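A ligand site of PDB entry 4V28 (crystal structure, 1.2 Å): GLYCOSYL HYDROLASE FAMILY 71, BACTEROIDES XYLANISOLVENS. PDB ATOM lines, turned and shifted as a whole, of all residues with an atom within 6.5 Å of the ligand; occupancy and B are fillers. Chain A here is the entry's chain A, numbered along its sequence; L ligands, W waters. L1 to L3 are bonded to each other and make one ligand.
An oxygen (O5) of LIG L1 lies within hydrogen-bond range of the guanidinium group (NH2) of Arg 295, at 2.9 Å. The side-chain amide nitrogen (NE2) of Gln 333 lies within hydrogen-bond range of an oxygen (O1) of LG2 L2 (2.9 Å). An oxygen (O5) of LG2 L2 sits at hydrogen-bond distance from the side-chain hydroxyl (OH) of Tyr 46 (2.7 Å). O5 of LG2 L2 is in hydrogen-bond range of OE2 of Glu 156, 2.7 Å away.
The side-chain carboxylate (OE2) of Glu 336 lies close to an oxygen (O4) of LG2 L2. Residues that only touch the ligand: Tyr 289, Trp 126, Phe 253, Tyr 195, Trp 48, His 154, Asn 298, Tyr 252, Phe 258, Ala 254, Ala 255 and Val 301. Hydrophobic or aromatic side chains within 4 Å of the ligand: Tyr 46, Trp 48, Trp 126, His 154, Tyr 195, Tyr 252, Phe 253, Ala 255, Phe 258, Tyr 289 and Val 301. Of the 29 residues printed, 17 come within 4 Å of the ligand. The nearest printed residue that does not touch the ligand is His 63 (4.01 Å).
Water W4 lies within hydrogen-bond range of a ring nitrogen (NE2) of His 63, an oxygen (O3) of LIG L1 and a ring nitrogen (ND1) of His 335. Water W8 bridges O3 of LIG L1 (2.9 Å) and NE2 of His 63 (3.4 Å). Water W3 lies within hydrogen-bond range of the side-chain carboxylate (OE1) of Glu 336 (2.8 Å), the backbone NH (N) of Ala 254 (2.9 Å) and an oxygen (O1) of LG3 L3 (3.0 Å).
The side-chain carboxylate (OE2) of Glu 336 is in hydrogen-bond range of the side-chain hydroxyl (OH) of Tyr 252 (2.5 Å). The side-chain hydroxyl (OG) of Ser 262 is in hydrogen-bond range of the backbone NH (N) of Phe 258 (3.4 Å). NE2 of His 154 is in hydrogen-bond range of OH of Tyr 250 (2.7 Å). The side-chain hydroxyl of Tyr 46 sits at hydrogen-bond distance from the side-chain hydroxyl of Tyr 252. The backbone NH of Tyr 195 lies close to the side-chain hydroxyl of Tyr 250, 3.2 Å away. OD1 of Asp 291 lies within hydrogen-bond range of ND2 of Asn 298 (3.1 Å). The side-chain hydroxyl (OH) of Tyr 289 lies within hydrogen-bond range of the side-chain carboxylate (OD2) of Asp 291 (2.7 Å). O of Ala 255 sits at hydrogen-bond distance from OG of Ser 262 (3.4 Å).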
ATOM      1  N   TYR A  46     -26.449  20.262 -10.419  1.00  0.00           N
ATOM      2  CA  TYR A  46     -25.398  20.975  -9.692  1.00  0.00           C
ATOM      3  C   TYR A  46     -24.131  20.942 -10.536  1.00  0.00           C
ATOM      4  O   TYR A  46     -23.731  19.901 -11.046  1.00  0.00           O
ATOM      5  CB  TYR A  46     -25.191  20.315  -8.332  1.00  0.00           C
ATOM      6  CG  TYR A  46     -26.340  20.574  -7.403  1.00  0.00           C
ATOM      7  CD1 TYR A  46     -27.554  19.901  -7.486  1.00  0.00           C
ATOM      8  CD2 TYR A  46     -26.165  21.527  -6.404  1.00  0.00           C
ATOM      9  CE1 TYR A  46     -28.594  20.239  -6.614  1.00  0.00           C
ATOM     10  CE2 TYR A  46     -27.134  21.809  -5.490  1.00  0.00           C
ATOM     11  CZ  TYR A  46     -28.349  21.205  -5.597  1.00  0.00           C
ATOM     12  OH  TYR A  46     -29.215  21.523  -4.568  1.00  0.00           O
ATOM     13  N   TRP A  48     -20.997  22.253  -9.465  1.00  0.00           N
ATOM     14  CA  TRP A  48     -19.967  22.695  -8.543  1.00  0.00           C
ATOM     15  C   TRP A  48     -18.847  21.670  -8.332  1.00  0.00           C
ATOM     16  O   TRP A  48     -18.004  21.867  -7.443  1.00  0.00           O
ATOM     17  CB  TRP A  48     -20.586  23.112  -7.215  1.00  0.00           C
ATOM     18  CG  TRP A  48     -21.413  22.063  -6.509  1.00  0.00           C
ATOM     19  CD1 TRP A  48     -21.389  20.704  -6.662  1.00  0.00           C
ATOM     20  CD2 TRP A  48     -22.327  22.332  -5.456  1.00  0.00           C
ATOM     21  NE1 TRP A  48     -22.257  20.124  -5.778  1.00  0.00           N
ATOM     22  CE2 TRP A  48     -22.839  21.095  -5.020  1.00  0.00           C
ATOM     23  CE3 TRP A  48     -22.745  23.490  -4.812  1.00  0.00           C
ATOM     24  CZ2 TRP A  48     -23.749  21.003  -3.979  1.00  0.00           C
ATOM     25  CZ3 TRP A  48     -23.626  23.388  -3.781  1.00  0.00           C
ATOM     26  CH2 TRP A  48     -24.128  22.169  -3.376  1.00  0.00           C
ATOM     27  N   HIS A  60     -15.800  20.077  -4.228  1.00  0.00           N
ATOM     28  CA  HIS A  60     -17.019  19.441  -3.753  1.00  0.00           C
ATOM     29  C   HIS A  60     -16.879  17.958  -3.412  1.00  0.00           C
ATOM     30  O   HIS A  60     -17.486  17.488  -2.420  1.00  0.00           O
ATOM     31  CB  HIS A  60     -18.248  19.822  -4.600  1.00  0.00           C
ATOM     32  CG  HIS A  60     -18.959  21.010  -4.049  1.00  0.00           C
ATOM     33  ND1 HIS A  60     -20.003  20.888  -3.173  1.00  0.00           N
ATOM     34  CD2 HIS A  60     -18.740  22.339  -4.182  1.00  0.00           C
ATOM     35  CE1 HIS A  60     -20.409  22.072  -2.791  1.00  0.00           C
ATOM     36  NE2 HIS A  60     -19.647  22.976  -3.378  1.00  0.00           N
ATOM     37  N   HIS A  63     -14.995  18.070   1.099  1.00  0.00           N
ATOM     38  CA  HIS A  63     -16.027  18.849   1.759  1.00  0.00           C
ATOM     39  C   HIS A  63     -15.845  18.857   3.276  1.00  0.00           C
ATOM     40  O   HIS A  63     -15.505  17.830   3.869  1.00  0.00           O
ATOM     41  CB  HIS A  63     -17.369  18.201   1.417  1.00  0.00           C
ATOM     42  CG  HIS A  63     -18.567  19.082   1.576  1.00  0.00           C
ATOM     43  ND1 HIS A  63     -19.078  19.476   2.802  1.00  0.00           N
ATOM     44  CD2 HIS A  63     -19.449  19.534   0.656  1.00  0.00           C
ATOM     45  CE1 HIS A  63     -20.183  20.161   2.617  1.00  0.00           C
ATOM     46  NE2 HIS A  63     -20.449  20.193   1.321  1.00  0.00           N
ATOM     47  N   THR A 124     -28.404  24.919 -10.840  1.00  0.00           N
ATOM     48  CA  THR A 124     -28.171  25.663  -9.631  1.00  0.00           C
ATOM     49  C   THR A 124     -27.296  26.881  -9.966  1.00  0.00           C
ATOM     50  O   THR A 124     -26.293  26.761 -10.669  1.00  0.00           O
ATOM     51  CB  THR A 124     -27.539  24.693  -8.598  1.00  0.00           C
ATOM     52  OG1 THR A 124     -28.450  23.596  -8.438  1.00  0.00           O
ATOM     53  CG2 THR A 124     -27.230  25.386  -7.229  1.00  0.00           C
ATOM     54  N   TRP A 126     -25.392  30.220  -8.232  1.00  0.00           N
ATOM     55  CA  TRP A 126     -24.823  30.660  -6.997  1.00  0.00           C
ATOM     56  C   TRP A 126     -24.364  32.147  -7.044  1.00  0.00           C
ATOM     57  O   TRP A 126     -23.903  32.684  -6.032  1.00  0.00           O
ATOM     58  CB  TRP A 126     -23.651  29.711  -6.691  1.00  0.00           C
ATOM     59  CG  TRP A 126     -24.107  28.262  -6.506  1.00  0.00           C
ATOM     60  CD1 TRP A 126     -23.917  27.221  -7.361  1.00  0.00           C
ATOM     61  CD2 TRP A 126     -24.829  27.736  -5.388  1.00  0.00           C
ATOM     62  NE1 TRP A 126     -24.477  26.077  -6.837  1.00  0.00           N
ATOM     63  CE2 TRP A 126     -25.068  26.368  -5.634  1.00  0.00           C
ATOM     64  CE3 TRP A 126     -25.324  28.308  -4.212  1.00  0.00           C
ATOM     65  CZ2 TRP A 126     -25.752  25.552  -4.733  1.00  0.00           C
ATOM     66  CZ3 TRP A 126     -25.999  27.500  -3.332  1.00  0.00           C
ATOM     67  CH2 TRP A 126     -26.208  26.133  -3.588  1.00  0.00           C
ATOM     68  N   HIS A 154     -31.995  27.780 -11.226  1.00  0.00           N
ATOM     69  CA  HIS A 154     -32.415  27.593  -9.843  1.00  0.00           C
ATOM     70  C   HIS A 154     -31.625  28.596  -9.023  1.00  0.00           C
ATOM     71  O   HIS A 154     -30.435  28.416  -8.766  1.00  0.00           O
ATOM     72  CB  HIS A 154     -32.134  26.165  -9.429  1.00  0.00           C
ATOM     73  CG  HIS A 154     -32.651  25.794  -8.074  1.00  0.00           C
ATOM     74  ND1 HIS A 154     -32.269  24.639  -7.455  1.00  0.00           N
ATOM     75  CD2 HIS A 154     -33.537  26.394  -7.238  1.00  0.00           C
ATOM     76  CE1 HIS A 154     -32.905  24.537  -6.301  1.00  0.00           C
ATOM     77  NE2 HIS A 154     -33.696  25.574  -6.151  1.00  0.00           N
ATOM     78  N   GLU A 156     -30.238  30.383  -6.125  1.00  0.00           N
ATOM     79  CA  GLU A 156     -29.906  30.065  -4.766  1.00  0.00           C
ATOM     80  C   GLU A 156     -29.749  31.321  -3.922  1.00  0.00           C
ATOM     81  O   GLU A 156     -29.618  32.428  -4.442  1.00  0.00           O
ATOM     82  CB  GLU A 156     -28.613  29.244  -4.750  1.00  0.00           C
ATOM     83  CG  GLU A 156     -28.746  27.935  -5.462  1.00  0.00           C
ATOM     84  CD  GLU A 156     -29.409  26.833  -4.658  1.00  0.00           C
ATOM     85  OE1 GLU A 156     -29.739  27.037  -3.487  1.00  0.00           O
ATOM     86  OE2 GLU A 156     -29.571  25.730  -5.249  1.00  0.00           O
ATOM     87  N   PRO A 157     -29.690  31.178  -2.584  1.00  0.00           N
ATOM     88  CA  PRO A 157     -29.530  32.337  -1.675  1.00  0.00           C
ATOM     89  C   PRO A 157     -28.099  32.852  -1.409  1.00  0.00           C
ATOM     90  O   PRO A 157     -27.505  32.460  -0.404  1.00  0.00           O
ATOM     91  CB  PRO A 157     -30.157  31.831  -0.371  1.00  0.00           C
ATOM     92  CG  PRO A 157     -30.039  30.358  -0.430  1.00  0.00           C
ATOM     93  CD  PRO A 157     -30.054  29.946  -1.872  1.00  0.00           C
ATOM     94  N   TYR A 195     -34.920  29.334  -4.483  1.00  0.00           N
ATOM     95  CA  TYR A 195     -34.726  28.617  -3.251  1.00  0.00           C
ATOM     96  C   TYR A 195     -34.756  29.576  -2.066  1.00  0.00           C
ATOM     97  O   TYR A 195     -34.243  30.681  -2.145  1.00  0.00           O
ATOM     98  CB  TYR A 195     -33.435  27.814  -3.266  1.00  0.00           C
ATOM     99  CG  TYR A 195     -33.330  26.883  -2.080  1.00  0.00           C
ATOM    100  CD1 TYR A 195     -34.023  25.693  -2.042  1.00  0.00           C
ATOM    101  CD2 TYR A 195     -32.562  27.201  -0.955  1.00  0.00           C
ATOM    102  CE1 TYR A 195     -33.971  24.837  -0.939  1.00  0.00           C
ATOM    103  CE2 TYR A 195     -32.481  26.364   0.126  1.00  0.00           C
ATOM    104  CZ  TYR A 195     -33.185  25.173   0.135  1.00  0.00           C
ATOM    105  OH  TYR A 195     -33.124  24.315   1.198  1.00  0.00           O
ATOM    106  N   ASP A 196     -35.400  29.171  -0.957  1.00  0.00           N
ATOM    107  CA  ASP A 196     -35.468  30.001   0.256  1.00  0.00           C
ATOM    108  C   ASP A 196     -36.124  31.340  -0.014  1.00  0.00           C
ATOM    109  O   ASP A 196     -35.810  32.357   0.608  1.00  0.00           O
ATOM    110  CB  ASP A 196     -34.083  30.213   0.879  1.00  0.00           C
ATOM    111  CG  ASP A 196     -33.750  29.228   1.920  1.00  0.00           C
ATOM    112  OD1 ASP A 196     -34.648  28.528   2.411  1.00  0.00           O
ATOM    113  OD2 ASP A 196     -32.549  29.163   2.262  1.00  0.00           O
ATOM    114  N   TYR A 250     -42.663  25.254  -5.692  1.00  0.00           N
ATOM    115  CA  TYR A 250     -42.064  23.931  -5.682  1.00  0.00           C
ATOM    116  C   TYR A 250     -41.680  23.617  -4.254  1.00  0.00           C
ATOM    117  O   TYR A 250     -41.777  24.451  -3.362  1.00  0.00           O
ATOM    118  CB  TYR A 250     -40.849  23.832  -6.631  1.00  0.00           C
ATOM    119  CG  TYR A 250     -39.565  24.494  -6.179  1.00  0.00           C
ATOM    120  CD1 TYR A 250     -39.505  25.851  -5.898  1.00  0.00           C
ATOM    121  CD2 TYR A 250     -38.391  23.776  -6.064  1.00  0.00           C
ATOM    122  CE1 TYR A 250     -38.342  26.459  -5.499  1.00  0.00           C
ATOM    123  CE2 TYR A 250     -37.189  24.373  -5.706  1.00  0.00           C
ATOM    124  CZ  TYR A 250     -37.168  25.710  -5.403  1.00  0.00           C
ATOM    125  OH  TYR A 250     -36.015  26.348  -5.005  1.00  0.00           O
ATOM    126  N   TYR A 252     -38.812  21.200  -3.380  1.00  0.00           N
ATOM    127  CA  TYR A 252     -37.406  20.790  -3.377  1.00  0.00           C
ATOM    128  C   TYR A 252     -37.078  19.479  -2.660  1.00  0.00           C
ATOM    129  O   TYR A 252     -36.493  18.587  -3.262  1.00  0.00           O
ATOM    130  CB  TYR A 252     -36.428  21.899  -2.919  1.00  0.00           C
ATOM    131  CG  TYR A 252     -34.998  21.457  -3.166  1.00  0.00           C
ATOM    132  CD1 TYR A 252     -34.464  21.461  -4.452  1.00  0.00           C
ATOM    133  CD2 TYR A 252     -34.232  20.928  -2.148  1.00  0.00           C
ATOM    134  CE1 TYR A 252     -33.213  20.956  -4.711  1.00  0.00           C
ATOM    135  CE2 TYR A 252     -32.962  20.414  -2.407  1.00  0.00           C
ATOM    136  CZ  TYR A 252     -32.457  20.418  -3.683  1.00  0.00           C
ATOM    137  OH  TYR A 252     -31.217  19.871  -3.970  1.00  0.00           O
ATOM    138  N   PHE A 253     -37.341  19.380  -1.355  1.00  0.00           N
ATOM    139  CA  PHE A 253     -36.685  18.347  -0.570  1.00  0.00           C
ATOM    140  C   PHE A 253     -37.079  16.947  -1.020  1.00  0.00           C
ATOM    141  O   PHE A 253     -38.257  16.614  -1.112  1.00  0.00           O
ATOM    142  CB  PHE A 253     -36.977  18.566   0.909  1.00  0.00           C
ATOM    143  CG  PHE A 253     -36.613  19.955   1.350  1.00  0.00           C
ATOM    144  CD1 PHE A 253     -35.288  20.366   1.354  1.00  0.00           C
ATOM    145  CD2 PHE A 253     -37.589  20.906   1.620  1.00  0.00           C
ATOM    146  CE1 PHE A 253     -34.937  21.667   1.640  1.00  0.00           C
ATOM    147  CE2 PHE A 253     -37.238  22.207   1.906  1.00  0.00           C
ATOM    148  CZ  PHE A 253     -35.912  22.578   1.921  1.00  0.00           C
ATOM    149  N   ALA A 254     -36.072  16.101  -1.216  1.00  0.00           N
ATOM    150  CA  ALA A 254     -36.305  14.727  -1.601  1.00  0.00           C
ATOM    151  C   ALA A 254     -36.761  13.856  -0.444  1.00  0.00           C
ATOM    152  O   ALA A 254     -37.293  12.785  -0.676  1.00  0.00           O
ATOM    153  CB  ALA A 254     -35.043  14.134  -2.217  1.00  0.00           C
ATOM    154  N   ALA A 255     -36.503  14.302   0.789  1.00  0.00           N
ATOM    155  CA  ALA A 255     -36.809  13.546   2.007  1.00  0.00           C
ATOM    156  C   ALA A 255     -38.241  13.807   2.434  1.00  0.00           C
ATOM    157  O   ALA A 255     -38.584  14.915   2.878  1.00  0.00           O
ATOM    158  CB  ALA A 255     -35.853  13.916   3.115  1.00  0.00           C
ATOM    159  N   THR A 256     -39.102  12.806   2.307  1.00  0.00           N
ATOM    160  CA  THR A 256     -40.495  12.983   2.646  1.00  0.00           C
ATOM    161  C   THR A 256     -40.630  13.394   4.112  1.00  0.00           C
ATOM    162  O   THR A 256     -39.968  12.827   4.993  1.00  0.00           O
ATOM    163  CB  THR A 256     -41.316  11.706   2.392  1.00  0.00           C
ATOM    164  OG1 THR A 256     -40.692  10.607   3.061  1.00  0.00           O
ATOM    165  CG2 THR A 256     -41.462  11.411   0.928  1.00  0.00           C
ATOM    166  N   PHE A 258     -39.758  16.161   5.532  1.00  0.00           N
ATOM    167  CA  PHE A 258     -38.787  17.151   6.017  1.00  0.00           C
ATOM    168  C   PHE A 258     -39.478  18.495   6.279  1.00  0.00           C
ATOM    169  O   PHE A 258     -39.140  19.179   7.247  1.00  0.00           O
ATOM    170  CB  PHE A 258     -37.605  17.281   5.057  1.00  0.00           C
ATOM    171  CG  PHE A 258     -36.503  18.192   5.532  1.00  0.00           C
ATOM    172  CD1 PHE A 258     -35.728  17.868   6.639  1.00  0.00           C
ATOM    173  CD2 PHE A 258     -36.228  19.375   4.865  1.00  0.00           C
ATOM    174  CE1 PHE A 258     -34.717  18.715   7.070  1.00  0.00           C
ATOM    175  CE2 PHE A 258     -35.207  20.211   5.266  1.00  0.00           C
ATOM    176  CZ  PHE A 258     -34.451  19.887   6.383  1.00  0.00           C
ATOM    177  N   SER A 262     -42.839  19.041   1.525  1.00  0.00           N
ATOM    178  CA  SER A 262     -42.245  17.794   1.050  1.00  0.00           C
ATOM    179  C   SER A 262     -42.892  16.564   1.670  1.00  0.00           C
ATOM    180  O   SER A 262     -42.296  15.513   1.707  1.00  0.00           O
ATOM    181  CB  SER A 262     -40.718  17.787   1.260  1.00  0.00           C
ATOM    182  OG  SER A 262     -40.361  17.810   2.621  1.00  0.00           O
ATOM    183  N   TYR A 289     -32.795   9.908   0.338  1.00  0.00           N
ATOM    184  CA  TYR A 289     -32.001  10.972   0.954  1.00  0.00           C
ATOM    185  C   TYR A 289     -31.054  10.355   1.971  1.00  0.00           C
ATOM    186  O   TYR A 289     -31.481   9.569   2.803  1.00  0.00           O
ATOM    187  CB  TYR A 289     -32.887  12.044   1.645  1.00  0.00           C
ATOM    188  CG  TYR A 289     -32.062  13.248   2.034  1.00  0.00           C
ATOM    189  CD1 TYR A 289     -31.359  13.278   3.235  1.00  0.00           C
ATOM    190  CD2 TYR A 289     -31.940  14.318   1.165  1.00  0.00           C
ATOM    191  CE1 TYR A 289     -30.545  14.376   3.539  1.00  0.00           C
ATOM    192  CE2 TYR A 289     -31.136  15.397   1.480  1.00  0.00           C
ATOM    193  CZ  TYR A 289     -30.423  15.415   2.642  1.00  0.00           C
ATOM    194  OH  TYR A 289     -29.611  16.500   2.876  1.00  0.00           O
ATOM    195  N   ASP A 291     -27.352  12.109   3.916  1.00  0.00           N
ATOM    196  CA  ASP A 291     -26.255  13.086   3.897  1.00  0.00           C
ATOM    197  C   ASP A 291     -25.280  12.907   5.052  1.00  0.00           C
ATOM    198  O   ASP A 291     -24.572  13.837   5.417  1.00  0.00           O
ATOM    199  CB  ASP A 291     -26.777  14.525   3.809  1.00  0.00           C
ATOM    200  CG  ASP A 291     -27.480  15.018   5.056  1.00  0.00           C
ATOM    201  OD1 ASP A 291     -27.582  14.285   6.057  1.00  0.00           O
ATOM    202  OD2 ASP A 291     -27.957  16.169   4.991  1.00  0.00           O
ATOM    203  N   ILE A 294     -21.416  14.018   5.302  1.00  0.00           N
ATOM    204  CA  ILE A 294     -21.155  15.391   5.647  1.00  0.00           C
ATOM    205  C   ILE A 294     -21.877  15.873   6.904  1.00  0.00           C
ATOM    206  O   ILE A 294     -21.444  16.870   7.494  1.00  0.00           O
ATOM    207  CB  ILE A 294     -21.371  16.381   4.471  1.00  0.00           C
ATOM    208  CG1 ILE A 294     -22.826  16.374   3.970  1.00  0.00           C
ATOM    209  CG2 ILE A 294     -20.418  16.057   3.320  1.00  0.00           C
ATOM    210  CD1 ILE A 294     -23.223  17.633   3.227  1.00  0.00           C
ATOM    211  N   ARG A 295     -22.937  15.188   7.328  1.00  0.00           N
ATOM    212  CA  ARG A 295     -23.687  15.518   8.554  1.00  0.00           C
ATOM    213  C   ARG A 295     -23.928  14.263   9.364  1.00  0.00           C
ATOM    214  O   ARG A 295     -25.022  13.683   9.303  1.00  0.00           O
ATOM    215  CB  ARG A 295     -25.016  16.142   8.218  1.00  0.00           C
ATOM    216  CG  ARG A 295     -24.973  17.460   7.510  1.00  0.00           C
ATOM    217  CD  ARG A 295     -26.383  18.016   7.430  1.00  0.00           C
ATOM    218  NE  ARG A 295     -26.326  19.352   6.901  1.00  0.00           N
ATOM    219  CZ  ARG A 295     -26.286  19.680   5.622  1.00  0.00           C
ATOM    220  NH1 ARG A 295     -26.451  18.778   4.659  1.00  0.00           N
ATOM    221  NH2 ARG A 295     -26.132  20.958   5.303  1.00  0.00           N
ATOM    222  N   ASN A 298     -27.168  13.701  11.313  1.00  0.00           N
ATOM    223  CA  ASN A 298     -28.441  13.989  10.642  1.00  0.00           C
ATOM    224  C   ASN A 298     -29.188  12.723  10.165  1.00  0.00           C
ATOM    225  O   ASN A 298     -29.916  12.762   9.161  1.00  0.00           O
ATOM    226  CB  ASN A 298     -28.186  14.936   9.466  1.00  0.00           C
ATOM    227  CG  ASN A 298     -29.409  15.677   9.032  1.00  0.00           C
ATOM    228  OD1 ASN A 298     -30.272  16.045   9.848  1.00  0.00           O
ATOM    229  ND2 ASN A 298     -29.498  15.952   7.748  1.00  0.00           N
ATOM    230  N   VAL A 301     -33.086  12.183   8.936  1.00  0.00           N
ATOM    231  CA  VAL A 301     -33.568  12.571   7.617  1.00  0.00           C
ATOM    232  C   VAL A 301     -33.303  11.491   6.552  1.00  0.00           C
ATOM    233  O   VAL A 301     -33.737  11.628   5.415  1.00  0.00           O
ATOM    234  CB  VAL A 301     -33.008  13.972   7.221  1.00  0.00           C
ATOM    235  CG1 VAL A 301     -33.611  14.490   5.940  1.00  0.00           C
ATOM    236  CG2 VAL A 301     -33.270  14.965   8.341  1.00  0.00           C
ATOM    237  N   THR A 329     -35.488  16.065  -7.560  1.00  0.00           N
ATOM    238  CA  THR A 329     -34.376  16.326  -6.662  1.00  0.00           C
ATOM    239  C   THR A 329     -33.701  14.997  -6.403  1.00  0.00           C
ATOM    240  O   THR A 329     -34.208  14.198  -5.618  1.00  0.00           O
ATOM    241  CB  THR A 329     -34.868  16.954  -5.358  1.00  0.00           C
ATOM    242  OG1 THR A 329     -35.545  18.158  -5.720  1.00  0.00           O
ATOM    243  CG2 THR A 329     -33.715  17.229  -4.411  1.00  0.00           C
ATOM    244  N   GLN A 333     -26.998  15.830  -6.757  1.00  0.00           N
ATOM    245  CA  GLN A 333     -26.629  16.341  -5.440  1.00  0.00           C
ATOM    246  C   GLN A 333     -26.110  15.138  -4.633  1.00  0.00           C
ATOM    247  O   GLN A 333     -26.840  14.473  -3.889  1.00  0.00           O
ATOM    248  CB  GLN A 333     -27.770  17.089  -4.766  1.00  0.00           C
ATOM    249  CG  GLN A 333     -27.319  18.391  -4.092  1.00  0.00           C
ATOM    250  CD  GLN A 333     -26.335  18.211  -2.968  1.00  0.00           C
ATOM    251  OE1 GLN A 333     -25.726  17.157  -2.801  1.00  0.00           O
ATOM    252  NE2 GLN A 333     -26.176  19.245  -2.162  1.00  0.00           N
ATOM    253  N   HIS A 335     -24.000  14.987  -2.239  1.00  0.00           N
ATOM    254  CA  HIS A 335     -23.892  15.141  -0.787  1.00  0.00           C
ATOM    255  C   HIS A 335     -25.188  14.755  -0.101  1.00  0.00           C
ATOM    256  O   HIS A 335     -25.160  14.210   1.007  1.00  0.00           O
ATOM    257  CB  HIS A 335     -23.560  16.588  -0.387  1.00  0.00           C
ATOM    258  CG  HIS A 335     -22.408  17.168  -1.139  1.00  0.00           C
ATOM    259  ND1 HIS A 335     -22.371  18.401  -1.742  1.00  0.00           N
ATOM    260  CD2 HIS A 335     -21.216  16.583  -1.382  1.00  0.00           C
ATOM    261  CE1 HIS A 335     -21.179  18.550  -2.323  1.00  0.00           C
ATOM    262  NE2 HIS A 335     -20.478  17.459  -2.117  1.00  0.00           N
ATOM    263  N   GLU A 336     -26.320  15.037  -0.746  1.00  0.00           N
ATOM    264  CA  GLU A 336     -27.675  14.759  -0.285  1.00  0.00           C
ATOM    265  C   GLU A 336     -28.038  13.306  -0.402  1.00  0.00           C
ATOM    266  O   GLU A 336     -28.986  12.872   0.206  1.00  0.00           O
ATOM    267  CB  GLU A 336     -28.720  15.470  -1.193  1.00  0.00           C
ATOM    268  CG  GLU A 336     -28.895  16.958  -1.023  1.00  0.00           C
ATOM    269  CD  GLU A 336     -29.949  17.579  -1.907  1.00  0.00           C
ATOM    270  OE1 GLU A 336     -30.865  16.919  -2.430  1.00  0.00           O
ATOM    271  OE2 GLU A 336     -29.910  18.813  -2.070  1.00  0.00           O
HETATM  272  C1  LIG L   1     -26.037  25.302  -0.005  1.00  0.00           C
HETATM  273  C2  LIG L   1     -24.655  25.813  -0.399  1.00  0.00           C
HETATM  274  C3  LIG L   1     -23.561  24.805  -0.058  1.00  0.00           C
HETATM  275  C4  LIG L   1     -23.656  24.477   1.424  1.00  0.00           C
HETATM  276  C5  LIG L   1     -25.071  23.981   1.747  1.00  0.00           C
HETATM  277  C6  LIG L   1     -25.276  23.671   3.221  1.00  0.00           C
HETATM  278  O1  LIG L   1     -24.423  27.051   0.264  1.00  0.00           O
HETATM  279  O2  LIG L   1     -22.316  25.391  -0.331  1.00  0.00           O
HETATM  280  O3  LIG L   1     -22.703  23.485   1.738  1.00  0.00           O
HETATM  281  O4  LIG L   1     -26.055  24.948   1.355  1.00  0.00           O
HETATM  282  O5  LIG L   1     -26.554  23.090   3.395  1.00  0.00           O
HETATM  283  C1  LG2 L   2     -28.954  21.526  -0.559  1.00  0.00           C
HETATM  284  C2  LG2 L   2     -27.610  22.150  -0.887  1.00  0.00           C
HETATM  285  C3  LG2 L   2     -27.673  23.645  -0.619  1.00  0.00           C
HETATM  286  C4  LG2 L   2     -28.767  24.276  -1.503  1.00  0.00           C
HETATM  287  C5  LG2 L   2     -30.092  23.524  -1.319  1.00  0.00           C
HETATM  288  C6  LG2 L   2     -31.048  23.907  -2.404  1.00  0.00           C
HETATM  289  O1  LG2 L   2     -27.385  21.865  -2.261  1.00  0.00           O
HETATM  290  O2  LG2 L   2     -26.407  24.202  -0.862  1.00  0.00           O
HETATM  291  O3  LG2 L   2     -28.957  25.650  -1.196  1.00  0.00           O
HETATM  292  O4  LG2 L   2     -29.974  22.101  -1.371  1.00  0.00           O
HETATM  293  O5  LG2 L   2     -30.583  23.747  -3.751  1.00  0.00           O
HETATM  294  C1  LG3 L   3     -30.042  20.006   3.834  1.00  0.00           C
HETATM  295  C2  LG3 L   3     -29.418  20.862   2.943  1.00  0.00           C
HETATM  296  C3  LG3 L   3     -29.826  20.940   1.618  1.00  0.00           C
HETATM  297  C4  LG3 L   3     -33.213  17.611   2.337  1.00  0.00           C
HETATM  298  C5  LG3 L   3     -32.863  17.514   3.705  1.00  0.00           C
HETATM  299  C6  LG3 L   3     -31.807  18.248   4.250  1.00  0.00           C
HETATM  300  O1  LG3 L   3     -34.159  16.950   1.795  1.00  0.00           O
HETATM  301  O2  LG3 L   3     -32.517  18.482   1.513  1.00  0.00           O
HETATM  302  C7  LG3 L   3     -31.406  18.125   5.688  1.00  0.00           C
HETATM  303  C8  LG3 L   3     -31.094  19.197   3.392  1.00  0.00           C
HETATM  304  C9  LG3 L   3     -31.504  19.282   1.997  1.00  0.00           C
HETATM  305  C10 LG3 L   3     -30.869  20.160   1.134  1.00  0.00           C
HETATM  306  O3  LG3 L   3     -29.169  21.822   0.835  1.00  0.00           O
HETATM  307  O   HOH W   1     -22.981  28.732  -1.402  1.00  0.00           O
HETATM  308  O   HOH W   2     -26.587  28.665   0.943  1.00  0.00           O
HETATM  309  O   HOH W   3     -33.348  16.951  -1.042  1.00  0.00           O
HETATM  310  O   HOH W   4     -22.500  21.303   0.079  1.00  0.00           O
HETATM  311  O   HOH W   5     -28.603  24.822   3.193  1.00  0.00           O
HETATM  312  O   HOH W   6     -28.876  26.923   1.223  1.00  0.00           O
HETATM  313  O   HOH W   7     -20.012  23.895   0.112  1.00  0.00           O
HETATM  314  O   HOH W   8     -23.016  21.119   3.377  1.00  0.00           O
